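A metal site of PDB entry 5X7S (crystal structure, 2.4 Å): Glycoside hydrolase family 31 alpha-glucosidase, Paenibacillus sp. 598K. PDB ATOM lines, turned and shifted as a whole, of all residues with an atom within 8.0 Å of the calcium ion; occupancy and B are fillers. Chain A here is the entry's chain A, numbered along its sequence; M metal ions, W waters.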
ATOM      1  N   HIS A 633      11.261  13.438   0.130  1.00  0.00           N
ATOM      2  CA  HIS A 633      10.435  14.017   1.215  1.00  0.00           C
ATOM      3  C   HIS A 633       9.772  12.960   2.088  1.00  0.00           C
ATOM      4  O   HIS A 633       9.336  13.258   3.190  1.00  0.00           O
ATOM      5  CB  HIS A 633       9.398  14.938   0.597  1.00  0.00           C
ATOM      6  CG  HIS A 633       9.977  16.048  -0.236  1.00  0.00           C
ATOM      7  ND1 HIS A 633      10.553  17.168   0.305  1.00  0.00           N
ATOM      8  CD2 HIS A 633      10.036  16.210  -1.576  1.00  0.00           C
ATOM      9  CE1 HIS A 633      10.945  17.978  -0.664  1.00  0.00           C
ATOM     10  NE2 HIS A 633      10.636  17.425  -1.822  1.00  0.00           N
ATOM     11  N   GLU A 973       4.778  21.010  14.021  1.00  0.00           N
ATOM     12  CA  GLU A 973       4.628  21.276  12.586  1.00  0.00           C
ATOM     13  C   GLU A 973       4.792  20.000  11.718  1.00  0.00           C
ATOM     14  O   GLU A 973       5.506  19.076  12.084  1.00  0.00           O
ATOM     15  CB  GLU A 973       5.611  22.375  12.097  1.00  0.00           C
ATOM     16  CG  GLU A 973       7.077  22.000  12.038  1.00  0.00           C
ATOM     17  CD  GLU A 973       7.948  23.197  11.673  1.00  0.00           C
ATOM     18  OE1 GLU A 973       8.078  23.495  10.463  1.00  0.00           O
ATOM     19  OE2 GLU A 973       8.456  23.863  12.602  1.00  0.00           O
ATOM     20  N   TYR A 974       4.115  19.995  10.584  1.00  0.00           N
ATOM     21  CA  TYR A 974       4.157  18.879   9.638  1.00  0.00           C
ATOM     22  C   TYR A 974       4.322  19.437   8.223  1.00  0.00           C
ATOM     23  O   TYR A 974       3.468  20.214   7.752  1.00  0.00           O
ATOM     24  CB  TYR A 974       2.910  18.011   9.769  1.00  0.00           C
ATOM     25  CG  TYR A 974       2.741  17.448  11.157  1.00  0.00           C
ATOM     26  CD1 TYR A 974       2.052  18.164  12.141  1.00  0.00           C
ATOM     27  CD2 TYR A 974       3.303  16.230  11.504  1.00  0.00           C
ATOM     28  CE1 TYR A 974       1.891  17.658  13.434  1.00  0.00           C
ATOM     29  CE2 TYR A 974       3.140  15.712  12.784  1.00  0.00           C
ATOM     30  CZ  TYR A 974       2.456  16.444  13.744  1.00  0.00           C
ATOM     31  OH  TYR A 974       2.322  15.943  15.018  1.00  0.00           O
ATOM     32  N   ALA A 975       5.431  19.060   7.548  1.00  0.00           N
ATOM     33  CA  ALA A 975       5.685  19.561   6.200  1.00  0.00           C
ATOM     34  C   ALA A 975       4.685  18.894   5.220  1.00  0.00           C
ATOM     35  O   ALA A 975       4.426  17.692   5.319  1.00  0.00           O
ATOM     36  CB  ALA A 975       7.146  19.310   5.814  1.00  0.00           C
ATOM     37  N   ALA A 976       4.079  19.659   4.316  1.00  0.00           N
ATOM     38  CA  ALA A 976       3.086  19.081   3.387  1.00  0.00           C
ATOM     39  C   ALA A 976       3.764  18.137   2.364  1.00  0.00           C
ATOM     40  O   ALA A 976       3.280  17.015   2.064  1.00  0.00           O
ATOM     41  CB  ALA A 976       2.290  20.162   2.680  1.00  0.00           C
ATOM     42  N   GLU A 977       4.884  18.603   1.845  1.00  0.00           N
ATOM     43  CA  GLU A 977       5.708  17.857   0.934  1.00  0.00           C
ATOM     44  C   GLU A 977       6.119  16.475   1.467  1.00  0.00           C
ATOM     45  O   GLU A 977       6.305  15.572   0.667  1.00  0.00           O
ATOM     46  CB  GLU A 977       6.929  18.681   0.560  1.00  0.00           C
ATOM     47  CG  GLU A 977       7.846  19.095   1.708  1.00  0.00           C
ATOM     48  CD  GLU A 977       7.597  20.500   2.238  1.00  0.00           C
ATOM     49  OE1 GLU A 977       6.443  20.986   2.184  1.00  0.00           O
ATOM     50  OE2 GLU A 977       8.570  21.142   2.764  1.00  0.00           O
ATOM     51  N   SER A 978       6.212  16.321   2.807  1.00  0.00           N
ATOM     52  CA  SER A 978       6.469  15.023   3.485  1.00  0.00           C
ATOM     53  C   SER A 978       5.211  14.199   3.842  1.00  0.00           C
ATOM     54  O   SER A 978       5.296  13.075   4.375  1.00  0.00           O
ATOM     55  CB  SER A 978       7.337  15.233   4.740  1.00  0.00           C
ATOM     56  OG  SER A 978       8.595  15.798   4.347  1.00  0.00           O
ATOM     57  N   SER A 988       6.606  20.514  -5.379  1.00  0.00           N
ATOM     58  CA  SER A 988       7.063  21.524  -6.327  1.00  0.00           C
ATOM     59  C   SER A 988       7.911  22.624  -5.646  1.00  0.00           C
ATOM     60  O   SER A 988       7.758  22.907  -4.434  1.00  0.00           O
ATOM     61  CB  SER A 988       5.837  22.098  -7.060  1.00  0.00           C
ATOM     62  OG  SER A 988       6.189  23.225  -7.829  1.00  0.00           O
ATOM     63  N   PHE A 993       8.545  31.673  -1.651  1.00  0.00           N
ATOM     64  CA  PHE A 993       8.206  31.866  -0.245  1.00  0.00           C
ATOM     65  C   PHE A 993       7.497  30.695   0.448  1.00  0.00           C
ATOM     66  O   PHE A 993       6.805  30.906   1.445  1.00  0.00           O
ATOM     67  CB  PHE A 993       7.445  33.181  -0.046  1.00  0.00           C
ATOM     68  CG  PHE A 993       8.240  34.414  -0.413  1.00  0.00           C
ATOM     69  CD1 PHE A 993       9.196  34.939   0.484  1.00  0.00           C
ATOM     70  CD2 PHE A 993       8.057  35.039  -1.627  1.00  0.00           C
ATOM     71  CE1 PHE A 993       9.934  36.077   0.130  1.00  0.00           C
ATOM     72  CE2 PHE A 993       8.806  36.164  -1.995  1.00  0.00           C
ATOM     73  CZ  PHE A 993       9.744  36.669  -1.107  1.00  0.00           C
ATOM     74  N   TYR A 994       7.649  29.488  -0.096  1.00  0.00           N
ATOM     75  CA  TYR A 994       7.333  28.261   0.633  1.00  0.00           C
ATOM     76  C   TYR A 994       8.385  28.049   1.734  1.00  0.00           C
ATOM     77  O   TYR A 994       9.534  28.604   1.695  1.00  0.00           O
ATOM     78  CB  TYR A 994       7.244  27.017  -0.285  1.00  0.00           C
ATOM     79  CG  TYR A 994       8.521  26.707  -1.035  1.00  0.00           C
ATOM     80  CD1 TYR A 994       9.566  26.010  -0.405  1.00  0.00           C
ATOM     81  CD2 TYR A 994       8.708  27.128  -2.341  1.00  0.00           C
ATOM     82  CE1 TYR A 994      10.765  25.758  -1.074  1.00  0.00           C
ATOM     83  CE2 TYR A 994       9.868  26.856  -3.023  1.00  0.00           C
ATOM     84  CZ  TYR A 994      10.924  26.172  -2.375  1.00  0.00           C
ATOM     85  OH  TYR A 994      12.111  25.888  -3.059  1.00  0.00           O
ATOM     86  N   LYS A 995       7.990  27.218   2.692  1.00  0.00           N
ATOM     87  CA  LYS A 995       8.795  26.827   3.829  1.00  0.00           C
ATOM     88  C   LYS A 995       9.403  25.467   3.584  1.00  0.00           C
ATOM     89  O   LYS A 995       8.926  24.729   2.734  1.00  0.00           O
ATOM     90  CB  LYS A 995       7.906  26.776   5.074  1.00  0.00           C
ATOM     91  CG  LYS A 995       7.259  28.098   5.451  1.00  0.00           C
ATOM     92  CD  LYS A 995       8.248  29.228   5.721  1.00  0.00           C
ATOM     93  CE  LYS A 995       7.526  30.573   5.737  1.00  0.00           C
ATOM     94  NZ  LYS A 995       8.290  31.626   6.464  1.00  0.00           N
ATOM     95  N   GLY A 996      10.444  25.130   4.316  1.00  0.00           N
ATOM     96  CA  GLY A 996      11.124  23.845   4.138  1.00  0.00           C
ATOM     97  C   GLY A 996      11.618  23.657   2.711  1.00  0.00           C
ATOM     98  O   GLY A 996      11.930  24.645   2.016  1.00  0.00           O
ATOM     99  N   ALA A 997      11.670  22.411   2.264  1.00  0.00           N
ATOM    100  CA  ALA A 997      12.301  22.068   0.963  1.00  0.00           C
ATOM    101  C   ALA A 997      11.376  22.201  -0.266  1.00  0.00           C
ATOM    102  O   ALA A 997      11.860  22.157  -1.410  1.00  0.00           O
ATOM    103  CB  ALA A 997      12.884  20.655   1.032  1.00  0.00           C
ATOM    104  N   ALA A 998      10.078  22.415  -0.041  1.00  0.00           N
ATOM    105  CA  ALA A 998       9.069  22.411  -1.140  1.00  0.00           C
ATOM    106  C   ALA A 998       7.649  22.718  -0.630  1.00  0.00           C
ATOM    107  O   ALA A 998       7.402  22.978   0.590  1.00  0.00           O
ATOM    108  CB  ALA A 998       9.061  21.045  -1.879  1.00  0.00           C
ATOM    109  N   PHE A 999       6.709  22.631  -1.568  1.00  0.00           N
ATOM    110  CA  PHE A 999       5.302  22.660  -1.209  1.00  0.00           C
ATOM    111  C   PHE A 999       4.454  21.652  -2.025  1.00  0.00           C
ATOM    112  O   PHE A 999       4.972  20.955  -2.903  1.00  0.00           O
ATOM    113  CB  PHE A 999       4.806  24.088  -1.342  1.00  0.00           C
ATOM    114  CG  PHE A 999       4.855  24.598  -2.735  1.00  0.00           C
ATOM    115  CD1 PHE A 999       3.795  24.368  -3.609  1.00  0.00           C
ATOM    116  CD2 PHE A 999       5.938  25.322  -3.171  1.00  0.00           C
ATOM    117  CE1 PHE A 999       3.839  24.853  -4.898  1.00  0.00           C
ATOM    118  CE2 PHE A 999       6.017  25.803  -4.471  1.00  0.00           C
ATOM    119  CZ  PHE A 999       4.955  25.563  -5.343  1.00  0.00           C
ATOM    120  N   VAL A1000       3.156  21.561  -1.736  1.00  0.00           N
ATOM    121  CA  VAL A1000       2.275  20.629  -2.464  1.00  0.00           C
ATOM    122  C   VAL A1000       1.327  21.374  -3.401  1.00  0.00           C
ATOM    123  O   VAL A1000       0.648  22.272  -2.961  1.00  0.00           O
ATOM    124  CB  VAL A1000       1.505  19.712  -1.525  1.00  0.00           C
ATOM    125  CG1 VAL A1000       0.523  18.876  -2.340  1.00  0.00           C
ATOM    126  CG2 VAL A1000       2.485  18.846  -0.705  1.00  0.00           C
ATOM    127  N   ARG A1027      -0.931  26.358   6.152  1.00  0.00           N
ATOM    128  CA  ARG A1027      -0.344  27.370   5.281  1.00  0.00           C
ATOM    129  C   ARG A1027      -0.622  26.984   3.830  1.00  0.00           C
ATOM    130  O   ARG A1027      -0.255  25.905   3.377  1.00  0.00           O
ATOM    131  CB  ARG A1027       1.163  27.557   5.549  1.00  0.00           C
ATOM    132  CG  ARG A1027       1.871  28.684   4.761  1.00  0.00           C
ATOM    133  CD  ARG A1027       3.317  28.884   5.287  1.00  0.00           C
ATOM    134  NE  ARG A1027       3.929  30.201   5.054  1.00  0.00           N
ATOM    135  CZ  ARG A1027       4.591  30.573   3.938  1.00  0.00           C
ATOM    136  NH1 ARG A1027       4.749  29.748   2.894  1.00  0.00           N
ATOM    137  NH2 ARG A1027       5.107  31.793   3.883  1.00  0.00           N
ATOM    138  N   TRP A1062       1.186  33.494   0.596  1.00  0.00           N
ATOM    139  CA  TRP A1062       0.798  32.386   1.475  1.00  0.00           C
ATOM    140  C   TRP A1062       0.048  32.901   2.711  1.00  0.00           C
ATOM    141  O   TRP A1062       0.507  33.808   3.397  1.00  0.00           O
ATOM    142  CB  TRP A1062       2.061  31.628   1.941  1.00  0.00           C
ATOM    143  CG  TRP A1062       2.842  31.067   0.816  1.00  0.00           C
ATOM    144  CD1 TRP A1062       3.824  31.685   0.092  1.00  0.00           C
ATOM    145  CD2 TRP A1062       2.710  29.749   0.266  1.00  0.00           C
ATOM    146  NE1 TRP A1062       4.324  30.825  -0.870  1.00  0.00           N
ATOM    147  CE2 TRP A1062       3.648  29.632  -0.790  1.00  0.00           C
ATOM    148  CE3 TRP A1062       1.891  28.649   0.560  1.00  0.00           C
ATOM    149  CZ2 TRP A1062       3.796  28.477  -1.528  1.00  0.00           C
ATOM    150  CZ3 TRP A1062       2.018  27.515  -0.185  1.00  0.00           C
ATOM    151  CH2 TRP A1062       2.974  27.428  -1.233  1.00  0.00           C
ATOM    152  N   LEU A1092      -0.553  23.685  -0.682  1.00  0.00           N
ATOM    153  CA  LEU A1092      -0.388  23.519   0.744  1.00  0.00           C
ATOM    154  C   LEU A1092       1.116  23.432   1.079  1.00  0.00           C
ATOM    155  O   LEU A1092       1.924  22.969   0.289  1.00  0.00           O
ATOM    156  CB  LEU A1092      -1.152  22.277   1.202  1.00  0.00           C
ATOM    157  CG  LEU A1092      -2.603  22.133   0.713  1.00  0.00           C
ATOM    158  CD1 LEU A1092      -3.098  20.797   1.221  1.00  0.00           C
ATOM    159  CD2 LEU A1092      -3.560  23.238   1.174  1.00  0.00           C
ATOM    160  N   ASP A1093       1.515  23.966   2.220  1.00  0.00           N
ATOM    161  CA  ASP A1093       2.935  24.076   2.538  1.00  0.00           C
ATOM    162  C   ASP A1093       3.243  23.373   3.840  1.00  0.00           C
ATOM    163  O   ASP A1093       4.255  22.699   3.924  1.00  0.00           O
ATOM    164  CB  ASP A1093       3.309  25.555   2.588  1.00  0.00           C
ATOM    165  CG  ASP A1093       4.831  25.816   2.606  1.00  0.00           C
ATOM    166  OD1 ASP A1093       5.647  25.019   2.098  1.00  0.00           O
ATOM    167  OD2 ASP A1093       5.214  26.869   3.137  1.00  0.00           O
ATOM    168  N   ARG A1094       2.369  23.521   4.862  1.00  0.00           N
ATOM    169  CA  ARG A1094       2.652  23.073   6.233  1.00  0.00           C
ATOM    170  C   ARG A1094       1.409  23.119   7.129  1.00  0.00           C
ATOM    171  O   ARG A1094       0.587  24.052   7.050  1.00  0.00           O
ATOM    172  CB  ARG A1094       3.767  23.972   6.856  1.00  0.00           C
ATOM    173  CG  ARG A1094       4.213  23.653   8.289  1.00  0.00           C
ATOM    174  CD  ARG A1094       3.463  24.457   9.362  1.00  0.00           C
ATOM    175  NE  ARG A1094       3.611  25.897   9.166  1.00  0.00           N
ATOM    176  CZ  ARG A1094       2.646  26.821   9.156  1.00  0.00           C
ATOM    177  NH1 ARG A1094       1.368  26.522   9.350  1.00  0.00           N
ATOM    178  NH2 ARG A1094       2.979  28.095   8.959  1.00  0.00           N
ATOM    179  N   LEU A1095       1.273  22.121   7.990  1.00  0.00           N
ATOM    180  CA  LEU A1095       0.203  22.056   8.980  1.00  0.00           C
ATOM    181  C   LEU A1095       0.812  22.191  10.344  1.00  0.00           C
ATOM    182  O   LEU A1095       1.695  21.369  10.731  1.00  0.00           O
ATOM    183  CB  LEU A1095      -0.516  20.705   8.929  1.00  0.00           C
ATOM    184  CG  LEU A1095      -1.700  20.585   9.906  1.00  0.00           C
ATOM    185  CD1 LEU A1095      -2.881  21.442   9.394  1.00  0.00           C
ATOM    186  CD2 LEU A1095      -2.098  19.146  10.113  1.00  0.00           C
ATOM    187  N   GLU A1108      10.397  29.256  10.799  1.00  0.00           N
ATOM    188  CA  GLU A1108       9.791  30.102   9.761  1.00  0.00           C
ATOM    189  C   GLU A1108       9.997  31.576  10.027  1.00  0.00           C
ATOM    190  O   GLU A1108       9.185  32.393   9.581  1.00  0.00           O
ATOM    191  CB  GLU A1108       8.273  29.846   9.706  1.00  0.00           C
ATOM    192  CG  GLU A1108       7.907  28.389   9.465  1.00  0.00           C
ATOM    193  CD  GLU A1108       6.429  28.183   9.160  1.00  0.00           C
ATOM    194  OE1 GLU A1108       5.596  29.146   9.272  1.00  0.00           O
ATOM    195  OE2 GLU A1108       6.086  27.023   8.811  1.00  0.00           O
HETATM  196 CA    CA M   1       6.818  23.304   3.039  1.00  0.00          CA
HETATM  197  O   HOH W   1       7.071  23.035   5.533  1.00  0.00           O
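The backbone carbonyl oxygen of Asp 1093 lies close to the backbone NH of Ala 976 (3.1 Å).
The guanidinium group (NH1) of Arg 1027 is in salt-bridge range of the side-chain carboxylate (OD2) of Asp 1093 (2.9 Å).
The side-chain carboxylate (OE2) of Glu 977 sits close to the backbone NH (N) of Ala 997 (3.4 Å).
The side-chain amino group (NZ) of Lys 995 is in hydrogen-bond range of the backbone carbonyl oxygen (O) of Glu 1108.
The calcium ion is bound by the side-chain carboxylate (OD1) of Asp 1093, the side-chain carboxylate (OE1) of Glu 977, water W1, the backbone carbonyl oxygen (O) of Ala 998, the backbone carbonyl oxygen (O) of Lys 995, the backbone carbonyl oxygen (O) of Asp 1093 and the side-chain carboxylate (OE2) of Glu 977.
The calcium ion has seven donor atoms within binding distance.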
